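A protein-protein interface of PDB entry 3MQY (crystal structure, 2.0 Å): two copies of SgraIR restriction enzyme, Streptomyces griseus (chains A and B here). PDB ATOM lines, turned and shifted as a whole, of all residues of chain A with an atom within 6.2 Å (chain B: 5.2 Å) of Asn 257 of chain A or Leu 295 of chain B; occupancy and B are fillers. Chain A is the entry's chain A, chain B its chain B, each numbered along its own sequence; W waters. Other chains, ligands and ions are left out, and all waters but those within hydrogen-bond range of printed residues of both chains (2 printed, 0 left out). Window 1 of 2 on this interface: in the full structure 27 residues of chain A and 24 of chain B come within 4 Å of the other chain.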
ATOM      1  N   LEU A 181      19.356  -5.628 -22.732  1.00  0.00           N
ATOM      2  CA  LEU A 181      20.254  -6.597 -23.378  1.00  0.00           C
ATOM      3  C   LEU A 181      21.554  -5.858 -23.832  1.00  0.00           C
ATOM      4  O   LEU A 181      21.671  -5.415 -24.952  1.00  0.00           O
ATOM      5  CB  LEU A 181      19.585  -7.345 -24.519  1.00  0.00           C
ATOM      6  CG  LEU A 181      20.283  -8.672 -24.910  1.00  0.00           C
ATOM      7  CD1 LEU A 181      20.101  -9.749 -23.853  1.00  0.00           C
ATOM      8  CD2 LEU A 181      19.826  -9.225 -26.250  1.00  0.00           C
ATOM      9  N   PRO A 252      33.374 -15.121 -24.495  1.00  0.00           N
ATOM     10  CA  PRO A 252      33.085 -15.207 -25.954  1.00  0.00           C
ATOM     11  C   PRO A 252      31.770 -16.003 -26.244  1.00  0.00           C
ATOM     12  O   PRO A 252      31.099 -15.754 -27.234  1.00  0.00           O
ATOM     13  CB  PRO A 252      34.228 -16.018 -26.521  1.00  0.00           C
ATOM     14  CG  PRO A 252      35.359 -15.971 -25.450  1.00  0.00           C
ATOM     15  CD  PRO A 252      34.703 -15.643 -24.120  1.00  0.00           C
ATOM     16  N   LEU A 253      31.494 -16.979 -25.396  1.00  0.00           N
ATOM     17  CA  LEU A 253      30.337 -17.845 -25.599  1.00  0.00           C
ATOM     18  C   LEU A 253      29.043 -17.052 -25.430  1.00  0.00           C
ATOM     19  O   LEU A 253      28.085 -17.199 -26.218  1.00  0.00           O
ATOM     20  CB  LEU A 253      30.431 -19.081 -24.698  1.00  0.00           C
ATOM     21  CG  LEU A 253      29.319 -20.160 -24.807  1.00  0.00           C
ATOM     22  CD1 LEU A 253      29.126 -20.666 -26.206  1.00  0.00           C
ATOM     23  CD2 LEU A 253      29.618 -21.336 -23.873  1.00  0.00           C
ATOM     24  N   TYR A 254      29.001 -16.227 -24.387  1.00  0.00           N
ATOM     25  CA  TYR A 254      27.891 -15.340 -24.138  1.00  0.00           C
ATOM     26  C   TYR A 254      27.796 -14.300 -25.198  1.00  0.00           C
ATOM     27  O   TYR A 254      26.719 -14.067 -25.788  1.00  0.00           O
ATOM     28  CB  TYR A 254      27.981 -14.649 -22.789  1.00  0.00           C
ATOM     29  CG  TYR A 254      26.757 -13.869 -22.497  1.00  0.00           C
ATOM     30  CD1 TYR A 254      25.560 -14.517 -22.195  1.00  0.00           C
ATOM     31  CD2 TYR A 254      26.743 -12.511 -22.597  1.00  0.00           C
ATOM     32  CE1 TYR A 254      24.390 -13.773 -21.920  1.00  0.00           C
ATOM     33  CE2 TYR A 254      25.618 -11.777 -22.359  1.00  0.00           C
ATOM     34  CZ  TYR A 254      24.416 -12.438 -22.033  1.00  0.00           C
ATOM     35  OH  TYR A 254      23.302 -11.686 -21.801  1.00  0.00           O
ATOM     36  N   GLU A 255      28.900 -13.648 -25.515  1.00  0.00           N
ATOM     37  CA  GLU A 255      28.751 -12.605 -26.522  1.00  0.00           C
ATOM     38  C   GLU A 255      28.310 -13.111 -27.889  1.00  0.00           C
ATOM     39  O   GLU A 255      27.613 -12.359 -28.584  1.00  0.00           O
ATOM     40  CB  GLU A 255      30.018 -11.752 -26.667  1.00  0.00           C
ATOM     41  CG  GLU A 255      29.763 -10.450 -27.358  1.00  0.00           C
ATOM     42  CD  GLU A 255      28.806  -9.487 -26.566  1.00  0.00           C
ATOM     43  OE1 GLU A 255      28.253  -8.587 -27.195  1.00  0.00           O
ATOM     44  OE2 GLU A 255      28.607  -9.633 -25.351  1.00  0.00           O
ATOM     45  N   ALA A 256      28.813 -14.296 -28.300  1.00  0.00           N
ATOM     46  CA  ALA A 256      28.506 -14.890 -29.569  1.00  0.00           C
ATOM     47  C   ALA A 256      26.982 -15.153 -29.642  1.00  0.00           C
ATOM     48  O   ALA A 256      26.379 -14.890 -30.645  1.00  0.00           O
ATOM     49  CB  ALA A 256      29.261 -16.242 -29.742  1.00  0.00           C
ATOM     50  N   ASN A 257      26.420 -15.654 -28.557  1.00  0.00           N
ATOM     51  CA  ASN A 257      24.949 -15.820 -28.391  1.00  0.00           C
ATOM     52  C   ASN A 257      24.206 -14.517 -28.507  1.00  0.00           C
ATOM     53  O   ASN A 257      23.071 -14.510 -29.045  1.00  0.00           O
ATOM     54  CB  ASN A 257      24.598 -16.458 -27.034  1.00  0.00           C
ATOM     55  CG  ASN A 257      24.637 -17.957 -27.070  1.00  0.00           C
ATOM     56  OD1 ASN A 257      23.661 -18.678 -27.502  1.00  0.00           O
ATOM     57  ND2 ASN A 257      25.723 -18.484 -26.564  1.00  0.00           N
ATOM     58  N   VAL A 258      24.824 -13.391 -28.091  1.00  0.00           N
ATOM     59  CA  VAL A 258      24.087 -12.108 -28.139  1.00  0.00           C
ATOM     60  C   VAL A 258      24.172 -11.586 -29.567  1.00  0.00           C
ATOM     61  O   VAL A 258      23.236 -10.993 -30.091  1.00  0.00           O
ATOM     62  CB  VAL A 258      24.574 -11.071 -27.109  1.00  0.00           C
ATOM     63  CG1 VAL A 258      23.975  -9.660 -27.399  1.00  0.00           C
ATOM     64  CG2 VAL A 258      24.178 -11.498 -25.709  1.00  0.00           C
ATOM     65  N   MET A 259      25.283 -11.857 -30.232  1.00  0.00           N
ATOM     66  CA  MET A 259      25.450 -11.373 -31.597  1.00  0.00           C
ATOM     67  C   MET A 259      24.471 -12.166 -32.481  1.00  0.00           C
ATOM     68  O   MET A 259      23.892 -11.619 -33.346  1.00  0.00           O
ATOM     69  CB  MET A 259      26.881 -11.557 -32.107  1.00  0.00           C
ATOM     70  CG  MET A 259      27.893 -10.660 -31.329  1.00  0.00           C
ATOM     71  SD  MET A 259      29.517 -10.746 -32.081  1.00  0.00           S
ATOM     72  CE  MET A 259      29.386  -9.772 -33.566  1.00  0.00           C
ATOM     73  N   GLN A 260      24.330 -13.444 -32.223  1.00  0.00           N
ATOM     74  CA  GLN A 260      23.416 -14.286 -32.980  1.00  0.00           C
ATOM     75  C   GLN A 260      21.977 -13.921 -32.787  1.00  0.00           C
ATOM     76  O   GLN A 260      21.293 -13.680 -33.772  1.00  0.00           O
ATOM     77  CB  GLN A 260      23.670 -15.733 -32.690  1.00  0.00           C
ATOM     78  CG  GLN A 260      24.957 -16.098 -33.401  1.00  0.00           C
ATOM     79  CD  GLN A 260      25.451 -17.366 -32.947  1.00  0.00           C
ATOM     80  OE1 GLN A 260      25.070 -17.801 -31.888  1.00  0.00           O
ATOM     81  NE2 GLN A 260      26.315 -17.999 -33.737  1.00  0.00           N
ATOM     82  N   LEU A 261      21.547 -13.785 -31.551  1.00  0.00           N
ATOM     83  CA  LEU A 261      20.221 -13.245 -31.268  1.00  0.00           C
ATOM     84  C   LEU A 261      19.941 -11.919 -31.974  1.00  0.00           C
ATOM     85  O   LEU A 261      18.897 -11.791 -32.655  1.00  0.00           O
ATOM     86  CB  LEU A 261      19.948 -13.132 -29.757  1.00  0.00           C
ATOM     87  CG  LEU A 261      18.574 -12.687 -29.217  1.00  0.00           C
ATOM     88  CD1 LEU A 261      18.527 -12.867 -27.688  1.00  0.00           C
ATOM     89  CD2 LEU A 261      18.213 -11.295 -29.467  1.00  0.00           C
ATOM     90  N   LEU A 262      20.831 -10.923 -31.834  1.00  0.00           N
ATOM     91  CA  LEU A 262      20.525  -9.615 -32.430  1.00  0.00           C
ATOM     92  C   LEU A 262      20.703  -9.604 -33.982  1.00  0.00           C
ATOM     93  O   LEU A 262      19.800  -9.168 -34.703  1.00  0.00           O
ATOM     94  CB  LEU A 262      21.251  -8.432 -31.743  1.00  0.00           C
ATOM     95  CG  LEU A 262      21.024  -8.120 -30.248  1.00  0.00           C
ATOM     96  CD1 LEU A 262      22.130  -7.104 -29.630  1.00  0.00           C
ATOM     97  CD2 LEU A 262      19.631  -7.583 -29.997  1.00  0.00           C
ATOM     98  N   PHE A 274      31.831 -16.861 -35.370  1.00  0.00           N
ATOM     99  CA  PHE A 274      32.555 -16.396 -34.194  1.00  0.00           C
ATOM    100  C   PHE A 274      33.472 -17.506 -33.746  1.00  0.00           C
ATOM    101  O   PHE A 274      33.025 -18.603 -33.472  1.00  0.00           O
ATOM    102  CB  PHE A 274      31.560 -16.049 -33.082  1.00  0.00           C
ATOM    103  CG  PHE A 274      32.126 -15.187 -31.961  1.00  0.00           C
ATOM    104  CD1 PHE A 274      31.387 -14.114 -31.467  1.00  0.00           C
ATOM    105  CD2 PHE A 274      33.362 -15.445 -31.387  1.00  0.00           C
ATOM    106  CE1 PHE A 274      31.845 -13.339 -30.457  1.00  0.00           C
ATOM    107  CE2 PHE A 274      33.811 -14.680 -30.326  1.00  0.00           C
ATOM    108  CZ  PHE A 274      33.052 -13.611 -29.868  1.00  0.00           C
ATOM    109  N   ALA A 293      25.200 -25.345 -28.642  1.00  0.00           N
ATOM    110  CA  ALA A 293      24.295 -24.742 -29.545  1.00  0.00           C
ATOM    111  C   ALA A 293      23.938 -23.336 -29.091  1.00  0.00           C
ATOM    112  O   ALA A 293      23.739 -23.071 -27.898  1.00  0.00           O
ATOM    113  CB  ALA A 293      22.979 -25.626 -29.676  1.00  0.00           C
ATOM    114  N   SER A 294      23.796 -22.469 -30.083  1.00  0.00           N
ATOM    115  CA  SER A 294      23.263 -21.144 -29.939  1.00  0.00           C
ATOM    116  C   SER A 294      21.863 -21.154 -29.366  1.00  0.00           C
ATOM    117  O   SER A 294      20.950 -21.827 -29.945  1.00  0.00           O
ATOM    118  CB  SER A 294      23.241 -20.463 -31.299  1.00  0.00           C
ATOM    119  OG  SER A 294      22.976 -19.071 -31.162  1.00  0.00           O
ATOM    120  N   LEU A 295      21.669 -20.390 -28.276  1.00  0.00           N
ATOM    121  CA  LEU A 295      20.460 -20.505 -27.470  1.00  0.00           C
ATOM    122  C   LEU A 295      19.205 -20.017 -28.211  1.00  0.00           C
ATOM    123  O   LEU A 295      18.120 -20.601 -28.042  1.00  0.00           O
ATOM    124  CB  LEU A 295      20.596 -19.818 -26.097  1.00  0.00           C
ATOM    125  CG  LEU A 295      21.716 -20.209 -25.093  1.00  0.00           C
ATOM    126  CD1 LEU A 295      21.508 -19.582 -23.717  1.00  0.00           C
ATOM    127  CD2 LEU A 295      21.947 -21.692 -24.910  1.00  0.00           C
ATOM    128  N   TYR A 296      19.353 -18.966 -29.015  1.00  0.00           N
ATOM    129  CA  TYR A 296      18.214 -18.342 -29.628  1.00  0.00           C
ATOM    130  C   TYR A 296      17.500 -19.266 -30.617  1.00  0.00           C
ATOM    131  O   TYR A 296      16.281 -19.284 -30.674  1.00  0.00           O
ATOM    132  CB  TYR A 296      18.599 -17.065 -30.355  1.00  0.00           C
ATOM    133  CG  TYR A 296      17.392 -16.168 -30.648  1.00  0.00           C
ATOM    134  CD1 TYR A 296      16.793 -15.427 -29.623  1.00  0.00           C
ATOM    135  CD2 TYR A 296      16.854 -16.055 -31.948  1.00  0.00           C
ATOM    136  CE1 TYR A 296      15.706 -14.572 -29.861  1.00  0.00           C
ATOM    137  CE2 TYR A 296      15.753 -15.207 -32.203  1.00  0.00           C
ATOM    138  CZ  TYR A 296      15.172 -14.477 -31.144  1.00  0.00           C
ATOM    139  OH  TYR A 296      14.083 -13.638 -31.324  1.00  0.00           O
ATOM    140  N   ALA A 308      27.044 -21.654 -31.266  1.00  0.00           N
ATOM    141  CA  ALA A 308      27.377 -20.259 -30.926  1.00  0.00           C
ATOM    142  C   ALA A 308      28.798 -19.945 -31.372  1.00  0.00           C
ATOM    143  O   ALA A 308      29.050 -18.995 -32.131  1.00  0.00           O
ATOM    144  CB  ALA A 308      27.213 -20.007 -29.395  1.00  0.00           C
ATOM    145  N   TYR B 254      26.049 -16.922 -18.351  1.00  0.00           N
ATOM    146  CA  TYR B 254      25.792 -18.045 -19.216  1.00  0.00           C
ATOM    147  C   TYR B 254      25.083 -19.259 -18.519  1.00  0.00           C
ATOM    148  O   TYR B 254      24.029 -19.750 -19.000  1.00  0.00           O
ATOM    149  CB  TYR B 254      27.083 -18.474 -19.933  1.00  0.00           C
ATOM    150  CG  TYR B 254      26.800 -19.551 -20.918  1.00  0.00           C
ATOM    151  CD1 TYR B 254      26.228 -19.232 -22.128  1.00  0.00           C
ATOM    152  CD2 TYR B 254      27.049 -20.899 -20.620  1.00  0.00           C
ATOM    153  CE1 TYR B 254      25.933 -20.209 -23.072  1.00  0.00           C
ATOM    154  CE2 TYR B 254      26.711 -21.914 -21.540  1.00  0.00           C
ATOM    155  CZ  TYR B 254      26.150 -21.532 -22.785  1.00  0.00           C
ATOM    156  OH  TYR B 254      25.807 -22.441 -23.724  1.00  0.00           O
ATOM    157  N   ASN B 257      21.465 -18.776 -17.823  1.00  0.00           N
ATOM    158  CA  ASN B 257      20.692 -18.971 -19.051  1.00  0.00           C
ATOM    159  C   ASN B 257      20.387 -20.444 -19.414  1.00  0.00           C
ATOM    160  O   ASN B 257      19.203 -20.794 -19.740  1.00  0.00           O
ATOM    161  CB  ASN B 257      21.333 -18.254 -20.250  1.00  0.00           C
ATOM    162  CG  ASN B 257      20.935 -16.817 -20.334  1.00  0.00           C
ATOM    163  OD1 ASN B 257      19.864 -16.536 -20.819  1.00  0.00           O
ATOM    164  ND2 ASN B 257      21.813 -15.871 -19.885  1.00  0.00           N
ATOM    165  N   ALA B 293      18.182  -9.566 -19.917  1.00  0.00           N
ATOM    166  CA  ALA B 293      17.098 -10.577 -20.058  1.00  0.00           C
ATOM    167  C   ALA B 293      17.643 -11.968 -20.346  1.00  0.00           C
ATOM    168  O   ALA B 293      18.618 -12.150 -21.084  1.00  0.00           O
ATOM    169  CB  ALA B 293      16.098 -10.146 -21.159  1.00  0.00           C
ATOM    170  N   SER B 294      17.033 -12.984 -19.755  1.00  0.00           N
ATOM    171  CA  SER B 294      17.178 -14.355 -20.257  1.00  0.00           C
ATOM    172  C   SER B 294      17.120 -14.417 -21.811  1.00  0.00           C
ATOM    173  O   SER B 294      16.234 -13.811 -22.428  1.00  0.00           O
ATOM    174  CB  SER B 294      16.063 -15.243 -19.692  1.00  0.00           C
ATOM    175  OG  SER B 294      16.314 -16.581 -20.049  1.00  0.00           O
ATOM    176  N   LEU B 295      18.063 -15.148 -22.415  1.00  0.00           N
ATOM    177  CA  LEU B 295      18.172 -15.187 -23.858  1.00  0.00           C
ATOM    178  C   LEU B 295      17.088 -16.147 -24.327  1.00  0.00           C
ATOM    179  O   LEU B 295      16.482 -15.899 -25.339  1.00  0.00           O
ATOM    180  CB  LEU B 295      19.515 -15.691 -24.299  1.00  0.00           C
ATOM    181  CG  LEU B 295      20.740 -14.846 -23.918  1.00  0.00           C
ATOM    182  CD1 LEU B 295      21.928 -15.297 -24.741  1.00  0.00           C
ATOM    183  CD2 LEU B 295      20.505 -13.351 -24.115  1.00  0.00           C
ATOM    184  N   TYR B 296      16.953 -17.250 -23.580  1.00  0.00           N
ATOM    185  CA  TYR B 296      15.874 -18.264 -23.695  1.00  0.00           C
ATOM    186  C   TYR B 296      14.544 -17.554 -23.639  1.00  0.00           C
ATOM    187  O   TYR B 296      13.744 -17.649 -24.551  1.00  0.00           O
ATOM    188  CB  TYR B 296      15.972 -19.313 -22.553  1.00  0.00           C
ATOM    189  CG  TYR B 296      14.649 -19.854 -22.045  1.00  0.00           C
ATOM    190  CD1 TYR B 296      13.836 -20.650 -22.854  1.00  0.00           C
ATOM    191  CD2 TYR B 296      14.208 -19.577 -20.748  1.00  0.00           C
ATOM    192  CE1 TYR B 296      12.618 -21.148 -22.385  1.00  0.00           C
ATOM    193  CE2 TYR B 296      12.980 -20.070 -20.278  1.00  0.00           C
ATOM    194  CZ  TYR B 296      12.191 -20.838 -21.114  1.00  0.00           C
ATOM    195  OH  TYR B 296      10.988 -21.326 -20.677  1.00  0.00           O
ATOM    196  N   GLY B 297      14.378 -16.767 -22.584  1.00  0.00           N
ATOM    197  CA  GLY B 297      13.133 -16.018 -22.309  1.00  0.00           C
ATOM    198  C   GLY B 297      12.772 -15.180 -23.523  1.00  0.00           C
ATOM    199  O   GLY B 297      11.676 -15.341 -24.123  1.00  0.00           O
ATOM    200  N   LEU B 298      13.715 -14.360 -23.951  1.00  0.00           N
ATOM    201  CA  LEU B 298      13.570 -13.704 -25.256  1.00  0.00           C
ATOM    202  C   LEU B 298      13.282 -14.665 -26.459  1.00  0.00           C
ATOM    203  O   LEU B 298      12.445 -14.325 -27.270  1.00  0.00           O
ATOM    204  CB  LEU B 298      14.759 -12.799 -25.584  1.00  0.00           C
ATOM    205  CG  LEU B 298      15.107 -11.643 -24.639  1.00  0.00           C
ATOM    206  CD1 LEU B 298      16.475 -11.052 -25.048  1.00  0.00           C
ATOM    207  CD2 LEU B 298      14.037 -10.520 -24.482  1.00  0.00           C
ATOM    208  N   ALA B 299      13.988 -15.800 -26.589  1.00  0.00           N
ATOM    209  CA  ALA B 299      13.830 -16.632 -27.737  1.00  0.00           C
ATOM    210  C   ALA B 299      12.381 -17.220 -27.793  1.00  0.00           C
ATOM    211  O   ALA B 299      11.796 -17.289 -28.841  1.00  0.00           O
ATOM    212  CB  ALA B 299      14.875 -17.761 -27.757  1.00  0.00           C
ATOM    213  N   GLU B 300      11.828 -17.620 -26.648  1.00  0.00           N
ATOM    214  CA  GLU B 300      10.430 -18.156 -26.576  1.00  0.00           C
ATOM    215  C   GLU B 300       9.388 -17.027 -26.707  1.00  0.00           C
ATOM    216  O   GLU B 300       8.363 -17.208 -27.368  1.00  0.00           O
ATOM    217  CB  GLU B 300      10.190 -18.930 -25.269  1.00  0.00           C
ATOM    218  CG  GLU B 300      10.938 -20.243 -25.138  1.00  0.00           C
ATOM    219  CD  GLU B 300      10.462 -21.359 -26.097  1.00  0.00           C
ATOM    220  OE1 GLU B 300       9.405 -21.227 -26.779  1.00  0.00           O
ATOM    221  OE2 GLU B 300      11.161 -22.403 -26.154  1.00  0.00           O
HETATM  222  O   HOH W   1      25.594 -21.753 -26.386  1.00  0.00           O
HETATM  223  O   HOH W   2      21.165 -12.914 -20.454  1.00  0.00           O
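Water W1 lies within hydrogen-bond range of the backbone carbonyl oxygen (O) of Ala 293 of chain A (2.7 Å), the side-chain hydroxyl (OH) of Tyr 254 of chain B (2.8 Å) and the side-chain amide nitrogen (ND2) of Asn 257 of chain A (3.3 Å). Water W2 lies within hydrogen-bond range of the backbone carbonyl oxygen (O) of Ala 293 of chain B (2.7 Å), the side-chain hydroxyl (OH) of Tyr 254 of chain A (2.8 Å) and the side-chain amide nitrogen (ND2) of Asn 257 of chain B (3.1 Å).
Along chain B the printed residues that touch a printed residue of chain A span positions 254 to 299. Of the 18 printed residues of chain A, 7 touch a printed residue of chain B. Along chain A the printed residues that touch a printed residue of chain B span positions 181 to 296.
Tyr 254 of chain A touches Asn 257 of chain B, and with the chains exchanged Asn 257 of chain A touches Tyr 254 of chain B. Tyr 254 of chain A touches Leu 295 of chain B, but with the chains exchanged Leu 295 of chain A does not touch Tyr 254 of chain B (4.1 Å). Asn 257 of chain A touches Leu 295 of chain B, and with the chains exchanged Leu 295 of chain A touches Asn 257 of chain B. Positions printed for both chains: 254, 257, 293, 294, 295 and 296. Of the 10 pairs that touch across the chains among the printed residues, 4 have their exchanged pair printed and touching as well.
Asn 257 of chain A touches two residues of chain B. Gln 260 of chain A touches none of the printed residues of chain B. Of the printed residues of chain B, Leu 295 of chain A touches Asn 257 (3.7 Å). Of the printed residues of chain B, Tyr 296 of chain A touches Ala 299 (3.5 Å). Printed residues of chain A within 4 Å of Ala 293 of chain B: Leu 181. Printed residues of chain A within 4 Å of Leu 295 of chain B: Leu 181, Tyr 254 and Asn 257. Printed residues of chain A within 4 Å of Leu 298 of chain B: Leu 261 (3.8 Å). The nearest printed residue of chain B that does not touch Asn 257 of chain A is Asn 257 of chain B (7.6 Å). The nearest printed residue of chain A that does not touch Leu 295 of chain B is Leu 261 of chain A (4.1 Å).
ND2 of Asn 257 of chain A is in hydrogen-bond range of O of Leu 253 of chain A, 2.7 Å away. N of Leu 295 of chain A is in hydrogen-bond range of OD1 of Asn 257 of chain A, at 2.7 Å. OD1 of Asn 257 of chain B lies within hydrogen-bond range of N of Leu 295 of chain B (2.8 Å).
Ala 293 of chain B touches Leu 181 of chain A. Leu 295 of chain B touches Leu 181 of chain A. Tyr 254 of chain B touches Leu 253 of chain A (CZ to CD2, 3.6 Å). Tyr 254 of chain A touches Asn 257 of chain B (CE1 to ND2, 3.9 Å). OH of Tyr 254 of chain A touches CD2 of Leu 295 of chain B, at 3.99 Å. Asn 257 of chain A touches Tyr 254 of chain B. Asn 257 of chain A touches Leu 295 of chain B (CB to CD1, 3.7 Å). CD1 of Leu 298 of chain B touches CD1 of Leu 261 of chain A, at 3.8 Å. Asn 257 of chain B touches Leu 295 of chain A. CE1 of Tyr 296 of chain A touches CA of Ala 299 of chain B, at 3.5 Å.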
